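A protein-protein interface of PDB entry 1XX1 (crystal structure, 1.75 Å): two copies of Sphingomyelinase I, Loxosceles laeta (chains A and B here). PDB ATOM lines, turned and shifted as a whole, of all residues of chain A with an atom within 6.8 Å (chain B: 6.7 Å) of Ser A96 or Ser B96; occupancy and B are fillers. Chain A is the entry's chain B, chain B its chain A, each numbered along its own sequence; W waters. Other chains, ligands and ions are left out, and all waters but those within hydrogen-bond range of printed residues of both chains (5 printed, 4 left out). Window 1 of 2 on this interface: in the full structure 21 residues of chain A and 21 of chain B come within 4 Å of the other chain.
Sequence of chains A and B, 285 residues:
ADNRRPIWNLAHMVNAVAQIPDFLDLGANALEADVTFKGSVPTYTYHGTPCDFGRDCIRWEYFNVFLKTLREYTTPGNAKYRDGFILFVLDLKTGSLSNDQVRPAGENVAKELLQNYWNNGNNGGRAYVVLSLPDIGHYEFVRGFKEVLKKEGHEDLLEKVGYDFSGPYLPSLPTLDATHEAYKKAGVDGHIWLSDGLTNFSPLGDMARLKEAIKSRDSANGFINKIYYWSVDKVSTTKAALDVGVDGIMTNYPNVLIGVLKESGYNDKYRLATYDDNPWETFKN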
ATOM      1  N   THR A  36      15.241  -1.873 -12.352  1.00  0.00           N
ATOM      2  CA  THR A  36      15.323  -1.004 -13.510  1.00  0.00           C
ATOM      3  C   THR A  36      14.942  -1.789 -14.760  1.00  0.00           C
ATOM      4  O   THR A  36      15.134  -3.013 -14.826  1.00  0.00           O
ATOM      5  CB  THR A  36      16.729  -0.411 -13.667  1.00  0.00           C
ATOM      6  OG1 THR A  36      17.626  -1.408 -14.182  1.00  0.00           O
ATOM      7  CG2 THR A  36      17.194   0.216 -12.332  1.00  0.00           C
ATOM      8  N   PHE A  37      14.425  -1.071 -15.743  1.00  0.00           N
ATOM      9  CA  PHE A  37      13.996  -1.670 -16.997  1.00  0.00           C
ATOM     10  C   PHE A  37      14.735  -1.064 -18.137  1.00  0.00           C
ATOM     11  O   PHE A  37      15.044   0.134 -18.119  1.00  0.00           O
ATOM     12  CB  PHE A  37      12.518  -1.457 -17.179  1.00  0.00           C
ATOM     13  CG  PHE A  37      11.718  -2.351 -16.329  1.00  0.00           C
ATOM     14  CD1 PHE A  37      11.174  -3.516 -16.861  1.00  0.00           C
ATOM     15  CD2 PHE A  37      11.549  -2.069 -14.972  1.00  0.00           C
ATOM     16  CE1 PHE A  37      10.446  -4.371 -16.060  1.00  0.00           C
ATOM     17  CE2 PHE A  37      10.823  -2.921 -14.151  1.00  0.00           C
ATOM     18  CZ  PHE A  37      10.261  -4.073 -14.707  1.00  0.00           C
ATOM     19  N   LYS A  38      15.055  -1.915 -19.106  1.00  0.00           N
ATOM     20  CA  LYS A  38      15.492  -1.452 -20.413  1.00  0.00           C
ATOM     21  C   LYS A  38      14.380  -1.895 -21.328  1.00  0.00           C
ATOM     22  O   LYS A  38      14.213  -3.085 -21.591  1.00  0.00           O
ATOM     23  CB  LYS A  38      16.806  -2.118 -20.789  1.00  0.00           C
ATOM     24  CG  LYS A  38      17.979  -1.684 -19.908  1.00  0.00           C
ATOM     25  CD  LYS A  38      18.142  -0.179 -19.941  1.00  0.00           C
ATOM     26  CE  LYS A  38      19.461   0.262 -19.336  1.00  0.00           C
ATOM     27  NZ  LYS A  38      19.596   1.721 -19.732  1.00  0.00           N
ATOM     28  N   GLY A  39      13.542  -0.954 -21.738  1.00  0.00           N
ATOM     29  CA  GLY A  39      12.296  -1.332 -22.385  1.00  0.00           C
ATOM     30  C   GLY A  39      11.544  -2.200 -21.396  1.00  0.00           C
ATOM     31  O   GLY A  39      11.509  -1.912 -20.210  1.00  0.00           O
ATOM     32  N   SER A  40      10.940  -3.262 -21.891  1.00  0.00           N
ATOM     33  CA  SER A  40      10.150  -4.168 -21.055  1.00  0.00           C
ATOM     34  C   SER A  40      11.022  -5.167 -20.256  1.00  0.00           C
ATOM     35  O   SER A  40      10.497  -5.987 -19.520  1.00  0.00           O
ATOM     36  CB  SER A  40       9.205  -4.928 -21.961  1.00  0.00           C
ATOM     37  OG  SER A  40       9.990  -5.700 -22.841  1.00  0.00           O
ATOM     38  N   LYS A  93      10.650  -0.052 -11.695  1.00  0.00           N
ATOM     39  CA  LYS A  93      10.799   1.271 -12.292  1.00  0.00           C
ATOM     40  C   LYS A  93      10.230   1.279 -13.709  1.00  0.00           C
ATOM     41  O   LYS A  93      10.967   1.386 -14.687  1.00  0.00           O
ATOM     42  CB  LYS A  93      12.264   1.689 -12.231  1.00  0.00           C
ATOM     43  CG  LYS A  93      12.752   1.733 -10.782  1.00  0.00           C
ATOM     44  CD  LYS A  93      11.991   2.725  -9.945  1.00  0.00           C
ATOM     45  CE  LYS A  93      12.427   2.616  -8.497  1.00  0.00           C
ATOM     46  NZ  LYS A  93      11.866   3.763  -7.704  1.00  0.00           N
ATOM     47  N   THR A  94       8.909   1.154 -13.781  1.00  0.00           N
ATOM     48  CA  THR A  94       8.209   1.015 -15.072  1.00  0.00           C
ATOM     49  C   THR A  94       7.762   2.375 -15.596  1.00  0.00           C
ATOM     50  O   THR A  94       7.074   2.459 -16.619  1.00  0.00           O
ATOM     51  CB  THR A  94       6.959   0.142 -14.925  1.00  0.00           C
ATOM     52  OG1 THR A  94       6.128   0.725 -13.908  1.00  0.00           O
ATOM     53  CG2 THR A  94       7.342  -1.281 -14.521  1.00  0.00           C
ATOM     54  N   GLY A  95       8.152   3.442 -14.905  1.00  0.00           N
ATOM     55  CA  GLY A  95       7.656   4.790 -15.206  1.00  0.00           C
ATOM     56  C   GLY A  95       7.921   5.291 -16.616  1.00  0.00           C
ATOM     57  O   GLY A  95       7.270   6.240 -17.063  1.00  0.00           O
ATOM     58  N   SER A  96       8.868   4.700 -17.307  1.00  0.00           N
ATOM     59  CA  SER A  96       9.239   5.184 -18.641  1.00  0.00           C
ATOM     60  C   SER A  96       8.774   4.261 -19.732  1.00  0.00           C
ATOM     61  O   SER A  96       9.020   4.510 -20.920  1.00  0.00           O
ATOM     62  CB  SER A  96      10.745   5.430 -18.712  1.00  0.00           C
ATOM     63  OG  SER A  96      11.027   6.517 -17.865  1.00  0.00           O
ATOM     64  N   LEU A  97       8.071   3.191 -19.339  1.00  0.00           N
ATOM     65  CA  LEU A  97       7.632   2.225 -20.305  1.00  0.00           C
ATOM     66  C   LEU A  97       6.536   2.805 -21.180  1.00  0.00           C
ATOM     67  O   LEU A  97       5.628   3.457 -20.698  1.00  0.00           O
ATOM     68  CB  LEU A  97       7.062   0.976 -19.623  1.00  0.00           C
ATOM     69  CG  LEU A  97       8.027   0.084 -18.830  1.00  0.00           C
ATOM     70  CD1 LEU A  97       7.221  -1.027 -18.163  1.00  0.00           C
ATOM     71  CD2 LEU A  97       8.995  -0.541 -19.711  1.00  0.00           C
ATOM     72  N   SER A  98       6.603   2.478 -22.460  1.00  0.00           N
ATOM     73  CA  SER A  98       5.470   2.764 -23.333  1.00  0.00           C
ATOM     74  C   SER A  98       4.328   1.811 -22.950  1.00  0.00           C
ATOM     75  O   SER A  98       4.525   0.760 -22.310  1.00  0.00           O
ATOM     76  CB  SER A  98       5.858   2.542 -24.774  1.00  0.00           C
ATOM     77  OG  SER A  98       5.998   1.154 -25.013  1.00  0.00           O
ATOM     78  N   GLN A 101       4.870  -1.783 -23.635  1.00  0.00           N
ATOM     79  CA  GLN A 101       5.903  -2.471 -22.865  1.00  0.00           C
ATOM     80  C   GLN A 101       5.433  -2.918 -21.480  1.00  0.00           C
ATOM     81  O   GLN A 101       6.118  -3.696 -20.811  1.00  0.00           O
ATOM     82  CB  GLN A 101       7.129  -1.588 -22.737  1.00  0.00           C
ATOM     83  CG  GLN A 101       7.841  -1.385 -24.039  1.00  0.00           C
ATOM     84  CD  GLN A 101       8.931  -0.350 -23.927  1.00  0.00           C
ATOM     85  OE1 GLN A 101       8.784   0.656 -23.256  1.00  0.00           O
ATOM     86  NE2 GLN A 101      10.028  -0.617 -24.556  1.00  0.00           N
ATOM     87  N   PRO A 134       4.713   2.028  -9.973  1.00  0.00           N
ATOM     88  CA  PRO A 134       4.664   3.465  -9.752  1.00  0.00           C
ATOM     89  C   PRO A 134       3.528   4.159 -10.497  1.00  0.00           C
ATOM     90  O   PRO A 134       3.500   5.398 -10.556  1.00  0.00           O
ATOM     91  CB  PRO A 134       5.999   3.916 -10.334  1.00  0.00           C
ATOM     92  CG  PRO A 134       6.201   3.084 -11.430  1.00  0.00           C
ATOM     93  CD  PRO A 134       5.658   1.691 -11.045  1.00  0.00           C
ATOM     94  N   HIS A 138      -0.591   1.017 -14.636  1.00  0.00           N
ATOM     95  CA  HIS A 138       0.245  -0.092 -15.106  1.00  0.00           C
ATOM     96  C   HIS A 138      -0.296  -1.447 -14.682  1.00  0.00           C
ATOM     97  O   HIS A 138       0.444  -2.433 -14.609  1.00  0.00           O
ATOM     98  CB  HIS A 138       1.666   0.091 -14.596  1.00  0.00           C
ATOM     99  CG  HIS A 138       2.394   1.159 -15.328  1.00  0.00           C
ATOM    100  ND1 HIS A 138       3.726   1.431 -15.122  1.00  0.00           N
ATOM    101  CD2 HIS A 138       1.967   2.022 -16.286  1.00  0.00           C
ATOM    102  CE1 HIS A 138       4.090   2.421 -15.921  1.00  0.00           C
ATOM    103  NE2 HIS A 138       3.040   2.798 -16.637  1.00  0.00           N
ATOM    104  N   THR B  36      11.053  13.524 -19.164  1.00  0.00           N
ATOM    105  CA  THR B  36      10.676  12.119 -19.001  1.00  0.00           C
ATOM    106  C   THR B  36      10.179  11.555 -20.330  1.00  0.00           C
ATOM    107  O   THR B  36       9.726  12.289 -21.202  1.00  0.00           O
ATOM    108  CB  THR B  36       9.567  11.962 -17.953  1.00  0.00           C
ATOM    109  OG1 THR B  36       8.346  12.455 -18.528  1.00  0.00           O
ATOM    110  CG2 THR B  36       9.928  12.691 -16.640  1.00  0.00           C
ATOM    111  N   PHE B  37      10.245  10.244 -20.452  1.00  0.00           N
ATOM    112  CA  PHE B  37       9.847   9.559 -21.648  1.00  0.00           C
ATOM    113  C   PHE B  37       8.869   8.472 -21.317  1.00  0.00           C
ATOM    114  O   PHE B  37       8.894   7.898 -20.215  1.00  0.00           O
ATOM    115  CB  PHE B  37      11.053   8.944 -22.292  1.00  0.00           C
ATOM    116  CG  PHE B  37      11.884   9.926 -23.001  1.00  0.00           C
ATOM    117  CD1 PHE B  37      11.741  10.097 -24.380  1.00  0.00           C
ATOM    118  CD2 PHE B  37      12.790  10.723 -22.298  1.00  0.00           C
ATOM    119  CE1 PHE B  37      12.471  11.024 -25.044  1.00  0.00           C
ATOM    120  CE2 PHE B  37      13.571  11.684 -22.982  1.00  0.00           C
ATOM    121  CZ  PHE B  37      13.417  11.803 -24.348  1.00  0.00           C
ATOM    122  N   LYS B  38       7.972   8.250 -22.269  1.00  0.00           N
ATOM    123  CA  LYS B  38       7.091   7.096 -22.236  1.00  0.00           C
ATOM    124  C   LYS B  38       7.464   6.401 -23.492  1.00  0.00           C
ATOM    125  O   LYS B  38       7.114   6.859 -24.579  1.00  0.00           O
ATOM    126  CB  LYS B  38       5.656   7.543 -22.273  1.00  0.00           C
ATOM    127  CG  LYS B  38       5.236   8.164 -21.001  1.00  0.00           C
ATOM    128  CD  LYS B  38       5.157   7.116 -19.916  1.00  0.00           C
ATOM    129  CE  LYS B  38       4.680   7.720 -18.625  1.00  0.00           C
ATOM    130  NZ  LYS B  38       4.811   6.715 -17.545  1.00  0.00           N
ATOM    131  N   GLY B  39       8.230   5.327 -23.351  1.00  0.00           N
ATOM    132  CA  GLY B  39       8.941   4.738 -24.469  1.00  0.00           C
ATOM    133  C   GLY B  39       9.750   5.840 -25.107  1.00  0.00           C
ATOM    134  O   GLY B  39      10.446   6.570 -24.430  1.00  0.00           O
ATOM    135  N   SER B  40       9.629   6.008 -26.416  1.00  0.00           N
ATOM    136  CA  SER B  40      10.486   6.962 -27.107  1.00  0.00           C
ATOM    137  C   SER B  40       9.877   8.387 -27.137  1.00  0.00           C
ATOM    138  O   SER B  40      10.410   9.301 -27.760  1.00  0.00           O
ATOM    139  CB  SER B  40      10.766   6.416 -28.498  1.00  0.00           C
ATOM    140  OG  SER B  40       9.581   6.508 -29.235  1.00  0.00           O
ATOM    141  N   LYS B  93      15.682  11.764 -19.848  1.00  0.00           N
ATOM    142  CA  LYS B  93      15.608  10.579 -18.991  1.00  0.00           C
ATOM    143  C   LYS B  93      15.317   9.363 -19.846  1.00  0.00           C
ATOM    144  O   LYS B  93      14.238   8.780 -19.768  1.00  0.00           O
ATOM    145  CB  LYS B  93      14.554  10.795 -17.891  1.00  0.00           C
ATOM    146  CG  LYS B  93      14.885  12.054 -17.063  1.00  0.00           C
ATOM    147  CD  LYS B  93      16.206  11.902 -16.339  1.00  0.00           C
ATOM    148  CE  LYS B  93      16.340  12.985 -15.275  1.00  0.00           C
ATOM    149  NZ  LYS B  93      17.664  12.903 -14.612  1.00  0.00           N
ATOM    150  N   THR B  94      16.326   9.002 -20.632  1.00  0.00           N
ATOM    151  CA  THR B  94      16.257   7.919 -21.601  1.00  0.00           C
ATOM    152  C   THR B  94      16.780   6.604 -21.027  1.00  0.00           C
ATOM    153  O   THR B  94      16.844   5.607 -21.747  1.00  0.00           O
ATOM    154  CB  THR B  94      17.140   8.256 -22.811  1.00  0.00           C
ATOM    155  OG1 THR B  94      18.486   8.463 -22.356  1.00  0.00           O
ATOM    156  CG2 THR B  94      16.613   9.512 -23.540  1.00  0.00           C
ATOM    157  N   GLY B  95      17.147   6.620 -19.745  1.00  0.00           N
ATOM    158  CA  GLY B  95      17.784   5.481 -19.065  1.00  0.00           C
ATOM    159  C   GLY B  95      17.037   4.166 -19.147  1.00  0.00           C
ATOM    160  O   GLY B  95      17.661   3.100 -19.070  1.00  0.00           O
ATOM    161  N   SER B  96      15.733   4.228 -19.340  1.00  0.00           N
ATOM    162  CA  SER B  96      14.893   3.030 -19.421  1.00  0.00           C
ATOM    163  C   SER B  96      14.484   2.644 -20.837  1.00  0.00           C
ATOM    164  O   SER B  96      13.755   1.673 -21.027  1.00  0.00           O
ATOM    165  CB  SER B  96      13.647   3.214 -18.558  1.00  0.00           C
ATOM    166  OG  SER B  96      14.069   3.297 -17.224  1.00  0.00           O
ATOM    167  N   LEU B  97      14.940   3.400 -21.834  1.00  0.00           N
ATOM    168  CA  LEU B  97      14.596   3.097 -23.212  1.00  0.00           C
ATOM    169  C   LEU B  97      15.220   1.772 -23.646  1.00  0.00           C
ATOM    170  O   LEU B  97      16.339   1.457 -23.279  1.00  0.00           O
ATOM    171  CB  LEU B  97      15.089   4.214 -24.149  1.00  0.00           C
ATOM    172  CG  LEU B  97      14.415   5.595 -24.111  1.00  0.00           C
ATOM    173  CD1 LEU B  97      15.120   6.472 -25.122  1.00  0.00           C
ATOM    174  CD2 LEU B  97      13.000   5.493 -24.474  1.00  0.00           C
ATOM    175  N   SER B  98      14.495   0.999 -24.431  1.00  0.00           N
ATOM    176  CA  SER B  98      15.141  -0.107 -25.109  1.00  0.00           C
ATOM    177  C   SER B  98      16.119   0.493 -26.133  1.00  0.00           C
ATOM    178  O   SER B  98      15.934   1.627 -26.596  1.00  0.00           O
ATOM    179  CB  SER B  98      14.099  -0.961 -25.819  1.00  0.00           C
ATOM    180  OG  SER B  98      13.566  -0.256 -26.922  1.00  0.00           O
ATOM    181  N   GLN B 101      14.496   2.184 -28.982  1.00  0.00           N
ATOM    182  CA  GLN B 101      13.698   3.376 -28.737  1.00  0.00           C
ATOM    183  C   GLN B 101      14.557   4.627 -28.667  1.00  0.00           C
ATOM    184  O   GLN B 101      14.018   5.711 -28.602  1.00  0.00           O
ATOM    185  CB  GLN B 101      12.928   3.255 -27.435  1.00  0.00           C
ATOM    186  CG  GLN B 101      11.743   2.361 -27.514  1.00  0.00           C
ATOM    187  CD  GLN B 101      11.102   2.128 -26.169  1.00  0.00           C
ATOM    188  OE1 GLN B 101      11.785   1.956 -25.152  1.00  0.00           O
ATOM    189  NE2 GLN B 101       9.788   2.127 -26.152  1.00  0.00           N
ATOM    190  N   PRO B 134      22.041  10.319 -20.383  1.00  0.00           N
ATOM    191  CA  PRO B 134      22.535   9.646 -19.201  1.00  0.00           C
ATOM    192  C   PRO B 134      23.280   8.349 -19.531  1.00  0.00           C
ATOM    193  O   PRO B 134      23.613   7.583 -18.625  1.00  0.00           O
ATOM    194  CB  PRO B 134      21.235   9.348 -18.446  1.00  0.00           C
ATOM    195  CG  PRO B 134      20.306   8.931 -19.538  1.00  0.00           C
ATOM    196  CD  PRO B 134      20.662   9.912 -20.699  1.00  0.00           C
ATOM    197  N   HIS B 138      23.795   6.041 -25.780  1.00  0.00           N
ATOM    198  CA  HIS B 138      22.601   6.584 -26.398  1.00  0.00           C
ATOM    199  C   HIS B 138      22.891   7.567 -27.522  1.00  0.00           C
ATOM    200  O   HIS B 138      22.058   8.404 -27.878  1.00  0.00           O
ATOM    201  CB  HIS B 138      21.720   7.228 -25.341  1.00  0.00           C
ATOM    202  CG  HIS B 138      21.002   6.231 -24.503  1.00  0.00           C
ATOM    203  ND1 HIS B 138      20.016   6.588 -23.611  1.00  0.00           N
ATOM    204  CD2 HIS B 138      21.122   4.881 -24.427  1.00  0.00           C
ATOM    205  CE1 HIS B 138      19.570   5.494 -23.005  1.00  0.00           C
ATOM    206  NE2 HIS B 138      20.224   4.447 -23.483  1.00  0.00           N
HETATM  207  O   HOH W   1      11.806   8.922 -18.554  1.00  0.00           O
HETATM  208  O   HOH W   2      11.857   0.807 -19.533  1.00  0.00           O
HETATM  209  O   HOH W   3      11.265   5.583 -21.764  1.00  0.00           O
HETATM  210  O   HOH W   4      13.571   6.307 -20.113  1.00  0.00           O
HETATM  211  O   HOH W   5      13.705   1.503 -15.239  1.00  0.00           O
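OE1 of Gln B101 is in hydrogen-bond range of NE2 of Gln A101 (3.2 Å).
The side-chain hydroxyl of Ser B96 lies close to the backbone carbonyl oxygen of Phe A37 (3.4 Å).
O of Gly B95 lies within hydrogen-bond range of NZ of Lys A38, 2.5 Å away.
NZ of Lys B38 sits at hydrogen-bond distance from O of Gly A95, 2.6 Å away.
N of Gly A39 is in hydrogen-bond range of O of Ser B96, at 2.7 Å.
The backbone NH (N) of Gly B39 is in hydrogen-bond range of the backbone carbonyl oxygen (O) of Ser A96, 2.7 Å away.
N of Gly B39 lies close to N of Ser A98 (3.4 Å).
The backbone NH (N) of Gly A39 sits close to the backbone NH (N) of Ser B98, 3.5 Å away.
The backbone carbonyl oxygen (O) of Phe B37 sits close to the side-chain hydroxyl (OG) of Ser A96 (3.5 Å).
Water W2 lies within hydrogen-bond range of O of Ser B96 (2.6 Å) and O of Gly A39 (2.8 Å).
Water W4 lies within hydrogen-bond range of O of Lys B93 (2.6 Å), N of Ser B96 (3.1 Å) and OG of Ser A96 (3.4 Å).
Water W1 lies within hydrogen-bond range of the side-chain hydroxyl (OG) of Ser A96 (2.6 Å), the backbone carbonyl oxygen (O) of Lys B93 (2.7 Å) and the backbone NH (N) of Phe B37 (2.8 Å).
Water W3 lies within hydrogen-bond range of O of Ser A96 (2.6 Å) and O of Gly B39 (3.0 Å).
Water W5 lies within hydrogen-bond range of OG of Ser B96 (2.7 Å), N of Phe A37 (2.7 Å) and O of Lys A93 (2.8 Å).
N of Ser A98 is in hydrogen-bond range of OE1 of Gln A101 (3.0 Å).
N of Ser B98 lies within hydrogen-bond range of OE1 of Gln B101 (3.0 Å).
Phe A37 touches Ser B96, and with the chains exchanged Ser A96 touches Phe B37.
Lys A38 touches Gly B95, and with the chains exchanged Gly A95 touches Lys B38.
Gly A39 touches Leu B97, and with the chains exchanged Leu A97 touches Gly B39.
Gln B101 touches its own counterpart, Gln A101.
Positions printed for both chains: 36, 37, 38, 39, 40, 93, 94, 95, 96, 97, 98, 101, 134 and 138.
Ser A96 touches four residues of chain B.
Ser B96 touches four residues of chain A.
Of the printed residues of chain B, Ser A98 touches Gly B39.
Printed residues of chain B within 4 Å of Leu A97: Lys B38 and Gly B39.
The nearest printed residue of chain A that does not touch Gly B95 is Phe A37 (4.1 Å).
Of the 14 printed residues of chain B, 8 touch a printed residue of chain A.
Printed residues of chain B that touch a printed residue of chain A: Phe B37, Lys B38, Gly B39, Gly B95, Ser B96, Leu B97, Ser B98 and Gln B101.
Among the printed residues, no Asp or Glu carboxylate lies within 4 Å of a Lys or Arg side-chain nitrogen of the other chain.
O of Ser B96 touches CA of Lys A38 (3.6 Å).
N of Gly A39 touches C of Leu B97, at 3.7 Å.
Phe B37 touches Gly A95.
Lys B38 touches Ser A96.
Ser A96 touches Ser B96 (CB to CB, 3.7 Å).
O of Leu A97 touches CD of Lys B38, at 3.8 Å.
N of Gly B39 touches C of Leu A97, 3.7 Å away.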
